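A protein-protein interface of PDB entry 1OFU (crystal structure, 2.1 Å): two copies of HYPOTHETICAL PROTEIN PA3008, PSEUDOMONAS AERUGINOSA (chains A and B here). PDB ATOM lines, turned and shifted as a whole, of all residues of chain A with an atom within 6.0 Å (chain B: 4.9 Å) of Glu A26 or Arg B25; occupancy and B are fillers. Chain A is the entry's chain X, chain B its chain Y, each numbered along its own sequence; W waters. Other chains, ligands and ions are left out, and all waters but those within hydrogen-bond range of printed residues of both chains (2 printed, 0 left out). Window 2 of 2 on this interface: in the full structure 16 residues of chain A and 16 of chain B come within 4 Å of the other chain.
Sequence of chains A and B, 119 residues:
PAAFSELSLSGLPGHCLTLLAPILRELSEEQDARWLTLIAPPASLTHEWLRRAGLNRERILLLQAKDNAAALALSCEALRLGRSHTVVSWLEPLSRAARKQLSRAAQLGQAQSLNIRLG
Pro B22 touches its own counterpart, Pro A22.
Ile A23 touches Pro B22, but with the chains exchanged Pro A22 does not touch Ile B23 (4.01 Å).
Ile B23 touches its own counterpart, Ile A23.
Arg A25 touches Glu B26, and with the chains exchanged Glu A26 touches Arg B25.
10 positions are printed for both chains.
Of the 7 pairs that touch across the chains among the printed residues, 6 have their exchanged pair printed and touching as well.
Water W1 bridges the side-chain carboxylate (OE2) of Glu A26 and the guanidinium group (NE) of Arg B25.
Water W2 lies within hydrogen-bond range of NE of Arg A25 (2.5 Å) and OE2 of Glu B26 (2.6 Å).
Printed residues of chain B within 4 Å of Pro A22: Pro B22 (3.7 Å) and Glu B26 (3.9 Å).
Of the printed residues of chain B, Ile A23 touches Pro B22 and Ile B23.
Of the printed residues of chain B, Arg A25 touches Glu B26.
Of chain B, only Pro B22 and Arg B25 come within 4 Å of Glu A26.
Leu A27 touches none of the printed residues of chain B.
Ala B21 touches none of the printed residues of chain A.
Of the printed residues of chain A, Pro B22 touches Pro A22 (3.7 Å), Ile A23 (3.3 Å) and Glu A26 (3.1 Å).
Of the printed residues of chain A, Ile B23 touches Ile A23.
Arg B25 touches just one residue of chain A: Glu A26 (2.7 Å).
The nearest printed residue of chain A that does not touch Arg B25 is Pro A22 (6.9 Å).
The nearest printed residue of chain A that does not touch Pro B22 is Arg A25 (6.5 Å).
OG of Ser A28 lies within hydrogen-bond range of O of Arg A25 (2.7 Å).
OG of Ser B28 lies within hydrogen-bond range of O of Arg B25 (2.6 Å).
Printed residues of chain A that touch a printed residue of chain B: Pro A22, Ile A23, Arg A25 and Glu A26.
Hydrophobic or aromatic side chains of chain A that line the printed part of chain B: Pro A22 and Ile A23.
Of the 12 printed residues of chain B, 4 touch a printed residue of chain A.
Hydrophobic or aromatic side chains of chain B within 4 Å of the printed part of chain A: Pro B22 and Ile B23.
Among the printed residues, 7 pairs touch across the chains.
OE2 of Glu A26 is in salt-bridge range of NH1 of Arg B25 (2.7 Å).
The side-chain carboxylate (OE1) of Glu B26 lies within salt-bridge range of the guanidinium group (NH1) of Arg A25 (3.2 Å).
Pro B22 touches Pro A22 (O to CB, 3.7 Å).
CB of Pro A22 touches CB of Glu B26, 3.9 Å away.
CG of Pro B22 touches CD1 of Ile A23 (3.3 Å).
Ile A23 touches Ile B23 (CD1 to CG1, 3.6 Å).
Glu A26 touches Pro B22 (OE2 to CB, 3.1 Å).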
ATOM      1  N   ALA A  21       0.110  10.539 -13.286  1.00  0.00           N
ATOM      2  CA  ALA A  21      -0.631  10.812 -12.053  1.00  0.00           C
ATOM      3  C   ALA A  21      -0.348   9.887 -10.861  1.00  0.00           C
ATOM      4  O   ALA A  21      -0.081  10.360  -9.760  1.00  0.00           O
ATOM      5  CB  ALA A  21      -2.134  10.837 -12.349  1.00  0.00           C
ATOM      6  N   PRO A  22      -0.424   8.558 -11.055  1.00  0.00           N
ATOM      7  CA  PRO A  22      -0.156   7.666  -9.923  1.00  0.00           C
ATOM      8  C   PRO A  22       1.212   7.832  -9.252  1.00  0.00           C
ATOM      9  O   PRO A  22       1.333   7.662  -8.039  1.00  0.00           O
ATOM     10  CB  PRO A  22      -0.369   6.265 -10.519  1.00  0.00           C
ATOM     11  CG  PRO A  22      -0.192   6.470 -11.999  1.00  0.00           C
ATOM     12  CD  PRO A  22      -0.845   7.793 -12.241  1.00  0.00           C
ATOM     13  N   ILE A  23       2.234   8.167 -10.037  1.00  0.00           N
ATOM     14  CA  ILE A  23       3.589   8.373  -9.510  1.00  0.00           C
ATOM     15  C   ILE A  23       3.610   9.611  -8.612  1.00  0.00           C
ATOM     16  O   ILE A  23       4.073   9.567  -7.470  1.00  0.00           O
ATOM     17  CB  ILE A  23       4.618   8.608 -10.660  1.00  0.00           C
ATOM     18  CG1 ILE A  23       4.631   7.414 -11.613  1.00  0.00           C
ATOM     19  CG2 ILE A  23       6.011   8.832 -10.083  1.00  0.00           C
ATOM     20  CD1 ILE A  23       5.117   6.151 -10.980  1.00  0.00           C
ATOM     21  N   LEU A  24       3.108  10.719  -9.145  1.00  0.00           N
ATOM     22  CA  LEU A  24       3.067  11.983  -8.413  1.00  0.00           C
ATOM     23  C   LEU A  24       2.193  11.868  -7.172  1.00  0.00           C
ATOM     24  O   LEU A  24       2.505  12.423  -6.125  1.00  0.00           O
ATOM     25  CB  LEU A  24       2.534  13.098  -9.322  1.00  0.00           C
ATOM     26  CG  LEU A  24       3.357  13.363 -10.586  1.00  0.00           C
ATOM     27  CD1 LEU A  24       2.717  14.484 -11.413  1.00  0.00           C
ATOM     28  CD2 LEU A  24       4.773  13.734 -10.189  1.00  0.00           C
ATOM     29  N   ARG A  25       1.089  11.145  -7.295  1.00  0.00           N
ATOM     30  CA  ARG A  25       0.189  10.952  -6.166  1.00  0.00           C
ATOM     31  C   ARG A  25       0.942  10.211  -5.051  1.00  0.00           C
ATOM     32  O   ARG A  25       0.957  10.651  -3.902  1.00  0.00           O
ATOM     33  CB  ARG A  25      -1.038  10.165  -6.632  1.00  0.00           C
ATOM     34  CG  ARG A  25      -2.092   9.896  -5.573  1.00  0.00           C
ATOM     35  CD  ARG A  25      -3.429   9.580  -6.240  1.00  0.00           C
ATOM     36  NE  ARG A  25      -3.306   8.606  -7.327  1.00  0.00           N
ATOM     37  CZ  ARG A  25      -3.804   8.778  -8.551  1.00  0.00           C
ATOM     38  NH1 ARG A  25      -3.649   7.843  -9.473  1.00  0.00           N
ATOM     39  NH2 ARG A  25      -4.451   9.888  -8.865  1.00  0.00           N
ATOM     40  N   GLU A  26       1.596   9.106  -5.391  1.00  0.00           N
ATOM     41  CA  GLU A  26       2.342   8.355  -4.383  1.00  0.00           C
ATOM     42  C   GLU A  26       3.543   9.150  -3.872  1.00  0.00           C
ATOM     43  O   GLU A  26       3.873   9.118  -2.685  1.00  0.00           O
ATOM     44  CB  GLU A  26       2.796   7.014  -4.959  1.00  0.00           C
ATOM     45  CG  GLU A  26       3.594   6.170  -3.988  1.00  0.00           C
ATOM     46  CD  GLU A  26       3.327   4.687  -4.162  1.00  0.00           C
ATOM     47  OE1 GLU A  26       4.032   3.875  -3.528  1.00  0.00           O
ATOM     48  OE2 GLU A  26       2.406   4.335  -4.926  1.00  0.00           O
ATOM     49  N   LEU A  27       4.211   9.873  -4.760  1.00  0.00           N
ATOM     50  CA  LEU A  27       5.349  10.660  -4.308  1.00  0.00           C
ATOM     51  C   LEU A  27       4.912  11.698  -3.289  1.00  0.00           C
ATOM     52  O   LEU A  27       5.648  11.987  -2.347  1.00  0.00           O
ATOM     53  CB  LEU A  27       6.042  11.358  -5.482  1.00  0.00           C
ATOM     54  CG  LEU A  27       7.039  10.510  -6.269  1.00  0.00           C
ATOM     55  CD1 LEU A  27       7.620  11.329  -7.416  1.00  0.00           C
ATOM     56  CD2 LEU A  27       8.149  10.027  -5.331  1.00  0.00           C
ATOM     57  N   SER A  28       3.714  12.250  -3.461  1.00  0.00           N
ATOM     58  CA  SER A  28       3.245  13.275  -2.530  1.00  0.00           C
ATOM     59  C   SER A  28       2.892  12.723  -1.158  1.00  0.00           C
ATOM     60  O   SER A  28       2.642  13.484  -0.224  1.00  0.00           O
ATOM     61  CB  SER A  28       2.044  14.046  -3.110  1.00  0.00           C
ATOM     62  OG  SER A  28       0.876  13.251  -3.207  1.00  0.00           O
ATOM     63  N   GLU A  29       2.889  11.400  -1.028  1.00  0.00           N
ATOM     64  CA  GLU A  29       2.565  10.765   0.245  1.00  0.00           C
ATOM     65  C   GLU A  29       3.775  10.077   0.881  1.00  0.00           C
ATOM     66  O   GLU A  29       3.624   9.346   1.856  1.00  0.00           O
ATOM     67  CB  GLU A  29       1.443   9.740   0.050  1.00  0.00           C
ATOM     68  CG  GLU A  29       0.177  10.310  -0.571  1.00  0.00           C
ATOM     69  CD  GLU A  29      -0.636  11.128   0.408  1.00  0.00           C
ATOM     70  OE1 GLU A  29      -0.038  11.874   1.210  1.00  0.00           O
ATOM     71  OE2 GLU A  29      -1.881  11.033   0.373  1.00  0.00           O
ATOM     72  N   GLU A  30       4.967  10.297   0.334  1.00  0.00           N
ATOM     73  CA  GLU A  30       6.173   9.680   0.887  1.00  0.00           C
ATOM     74  C   GLU A  30       6.239   9.800   2.403  1.00  0.00           C
ATOM     75  O   GLU A  30       5.922  10.847   2.963  1.00  0.00           O
ATOM     76  CB  GLU A  30       7.430  10.309   0.286  1.00  0.00           C
ATOM     77  CG  GLU A  30       7.819   9.711  -1.039  1.00  0.00           C
ATOM     78  CD  GLU A  30       8.237   8.258  -0.905  1.00  0.00           C
ATOM     79  OE1 GLU A  30       8.298   7.559  -1.937  1.00  0.00           O
ATOM     80  OE2 GLU A  30       8.515   7.819   0.232  1.00  0.00           O
ATOM     81  N   LEU A  55      -3.223  14.391  -5.497  1.00  0.00           N
ATOM     82  CA  LEU A  55      -1.999  14.565  -4.726  1.00  0.00           C
ATOM     83  C   LEU A  55      -2.303  15.184  -3.365  1.00  0.00           C
ATOM     84  O   LEU A  55      -3.288  15.904  -3.202  1.00  0.00           O
ATOM     85  CB  LEU A  55      -1.009  15.466  -5.468  1.00  0.00           C
ATOM     86  CG  LEU A  55      -0.830  15.330  -6.982  1.00  0.00           C
ATOM     87  CD1 LEU A  55       0.538  15.880  -7.345  1.00  0.00           C
ATOM     88  CD2 LEU A  55      -0.936  13.887  -7.428  1.00  0.00           C
ATOM     89  N   ALA B  21       6.010   0.394  -9.590  1.00  0.00           N
ATOM     90  CA  ALA B  21       4.977  -0.103  -8.685  1.00  0.00           C
ATOM     91  C   ALA B  21       3.649   0.653  -8.620  1.00  0.00           C
ATOM     92  O   ALA B  21       2.584   0.049  -8.756  1.00  0.00           O
ATOM     93  CB  ALA B  21       5.562  -0.238  -7.285  1.00  0.00           C
ATOM     94  N   PRO B  22       3.686   1.977  -8.396  1.00  0.00           N
ATOM     95  CA  PRO B  22       2.426   2.723  -8.323  1.00  0.00           C
ATOM     96  C   PRO B  22       1.572   2.679  -9.583  1.00  0.00           C
ATOM     97  O   PRO B  22       0.345   2.735  -9.508  1.00  0.00           O
ATOM     98  CB  PRO B  22       2.878   4.145  -7.955  1.00  0.00           C
ATOM     99  CG  PRO B  22       4.291   4.205  -8.424  1.00  0.00           C
ATOM    100  CD  PRO B  22       4.834   2.849  -8.098  1.00  0.00           C
ATOM    101  N   ILE B  23       2.215   2.561 -10.740  1.00  0.00           N
ATOM    102  CA  ILE B  23       1.486   2.514 -12.001  1.00  0.00           C
ATOM    103  C   ILE B  23       0.826   1.149 -12.175  1.00  0.00           C
ATOM    104  O   ILE B  23      -0.341   1.049 -12.570  1.00  0.00           O
ATOM    105  CB  ILE B  23       2.438   2.786 -13.182  1.00  0.00           C
ATOM    106  CG1 ILE B  23       2.946   4.227 -13.099  1.00  0.00           C
ATOM    107  CG2 ILE B  23       1.728   2.523 -14.498  1.00  0.00           C
ATOM    108  CD1 ILE B  23       3.970   4.578 -14.141  1.00  0.00           C
ATOM    109  N   LEU B  24       1.580   0.097 -11.875  1.00  0.00           N
ATOM    110  CA  LEU B  24       1.058  -1.258 -11.984  1.00  0.00           C
ATOM    111  C   LEU B  24      -0.029  -1.445 -10.943  1.00  0.00           C
ATOM    112  O   LEU B  24      -1.052  -2.062 -11.205  1.00  0.00           O
ATOM    113  CB  LEU B  24       2.173  -2.281 -11.759  1.00  0.00           C
ATOM    114  CG  LEU B  24       3.182  -2.390 -12.897  1.00  0.00           C
ATOM    115  CD1 LEU B  24       4.103  -3.579 -12.642  1.00  0.00           C
ATOM    116  CD2 LEU B  24       2.445  -2.572 -14.216  1.00  0.00           C
ATOM    117  N   ARG B  25       0.204  -0.900  -9.756  1.00  0.00           N
ATOM    118  CA  ARG B  25      -0.753  -0.988  -8.663  1.00  0.00           C
ATOM    119  C   ARG B  25      -2.057  -0.311  -9.105  1.00  0.00           C
ATOM    120  O   ARG B  25      -3.138  -0.888  -9.012  1.00  0.00           O
ATOM    121  CB  ARG B  25      -0.141  -0.307  -7.435  1.00  0.00           C
ATOM    122  CG  ARG B  25      -0.916  -0.391  -6.134  1.00  0.00           C
ATOM    123  CD  ARG B  25       0.057  -0.302  -4.950  1.00  0.00           C
ATOM    124  NE  ARG B  25       1.014   0.800  -5.077  1.00  0.00           N
ATOM    125  CZ  ARG B  25       2.326   0.697  -4.854  1.00  0.00           C
ATOM    126  NH1 ARG B  25       3.113   1.754  -4.997  1.00  0.00           N
ATOM    127  NH2 ARG B  25       2.865  -0.461  -4.491  1.00  0.00           N
ATOM    128  N   GLU B  26      -1.937   0.908  -9.616  1.00  0.00           N
ATOM    129  CA  GLU B  26      -3.082   1.676 -10.091  1.00  0.00           C
ATOM    130  C   GLU B  26      -3.802   0.924 -11.210  1.00  0.00           C
ATOM    131  O   GLU B  26      -5.024   0.766 -11.190  1.00  0.00           O
ATOM    132  CB  GLU B  26      -2.602   3.043 -10.602  1.00  0.00           C
ATOM    133  CG  GLU B  26      -3.691   3.916 -11.213  1.00  0.00           C
ATOM    134  CD  GLU B  26      -4.474   4.706 -10.177  1.00  0.00           C
ATOM    135  OE1 GLU B  26      -5.452   5.381 -10.566  1.00  0.00           O
ATOM    136  OE2 GLU B  26      -4.110   4.659  -8.982  1.00  0.00           O
ATOM    137  N   LEU B  27      -3.040   0.466 -12.198  1.00  0.00           N
ATOM    138  CA  LEU B  27      -3.620  -0.275 -13.309  1.00  0.00           C
ATOM    139  C   LEU B  27      -4.383  -1.515 -12.840  1.00  0.00           C
ATOM    140  O   LEU B  27      -5.456  -1.824 -13.359  1.00  0.00           O
ATOM    141  CB  LEU B  27      -2.529  -0.691 -14.293  1.00  0.00           C
ATOM    142  CG  LEU B  27      -1.986   0.429 -15.175  1.00  0.00           C
ATOM    143  CD1 LEU B  27      -0.860  -0.109 -16.040  1.00  0.00           C
ATOM    144  CD2 LEU B  27      -3.120   0.991 -16.038  1.00  0.00           C
ATOM    145  N   SER B  28      -3.838  -2.219 -11.856  1.00  0.00           N
ATOM    146  CA  SER B  28      -4.494  -3.425 -11.369  1.00  0.00           C
ATOM    147  C   SER B  28      -5.865  -3.143 -10.757  1.00  0.00           C
ATOM    148  O   SER B  28      -6.674  -4.058 -10.588  1.00  0.00           O
ATOM    149  CB  SER B  28      -3.611  -4.140 -10.342  1.00  0.00           C
ATOM    150  OG  SER B  28      -3.594  -3.460  -9.101  1.00  0.00           O
ATOM    151  N   GLU B  29      -6.134  -1.879 -10.441  1.00  0.00           N
ATOM    152  CA  GLU B  29      -7.411  -1.506  -9.835  1.00  0.00           C
ATOM    153  C   GLU B  29      -8.377  -0.811 -10.799  1.00  0.00           C
ATOM    154  O   GLU B  29      -9.415  -0.306 -10.374  1.00  0.00           O
ATOM    155  CB  GLU B  29      -7.175  -0.581  -8.636  1.00  0.00           C
ATOM    156  CG  GLU B  29      -6.305  -1.155  -7.518  1.00  0.00           C
ATOM    157  CD  GLU B  29      -7.003  -2.234  -6.699  1.00  0.00           C
ATOM    158  OE1 GLU B  29      -8.223  -2.444  -6.881  1.00  0.00           O
ATOM    159  OE2 GLU B  29      -6.329  -2.867  -5.861  1.00  0.00           O
ATOM    160  N   ALA B  53       4.147  -5.393  -4.134  1.00  0.00           N
ATOM    161  CA  ALA B  53       3.880  -4.082  -4.717  1.00  0.00           C
ATOM    162  C   ALA B  53       2.418  -3.710  -4.465  1.00  0.00           C
ATOM    163  O   ALA B  53       1.967  -2.634  -4.844  1.00  0.00           O
ATOM    164  CB  ALA B  53       4.165  -4.102  -6.198  1.00  0.00           C
ATOM    165  N   GLY B  54       1.679  -4.616  -3.834  1.00  0.00           N
ATOM    166  CA  GLY B  54       0.284  -4.359  -3.520  1.00  0.00           C
ATOM    167  C   GLY B  54      -0.699  -4.401  -4.675  1.00  0.00           C
ATOM    168  O   GLY B  54      -1.789  -3.840  -4.571  1.00  0.00           O
ATOM    169  N   LEU B  55      -0.348  -5.057  -5.778  1.00  0.00           N
ATOM    170  CA  LEU B  55      -1.275  -5.120  -6.902  1.00  0.00           C
ATOM    171  C   LEU B  55      -2.498  -5.953  -6.517  1.00  0.00           C
ATOM    172  O   LEU B  55      -2.429  -6.800  -5.628  1.00  0.00           O
ATOM    173  CB  LEU B  55      -0.617  -5.752  -8.137  1.00  0.00           C
ATOM    174  CG  LEU B  55       0.753  -5.294  -8.648  1.00  0.00           C
ATOM    175  CD1 LEU B  55       0.843  -5.619 -10.128  1.00  0.00           C
ATOM    176  CD2 LEU B  55       0.946  -3.809  -8.437  1.00  0.00           C
HETATM  177  O   HOH W   1       0.180   3.341  -5.164  1.00  0.00           O
HETATM  178  O   HOH W   2      -2.614   6.243  -7.517  1.00  0.00           O
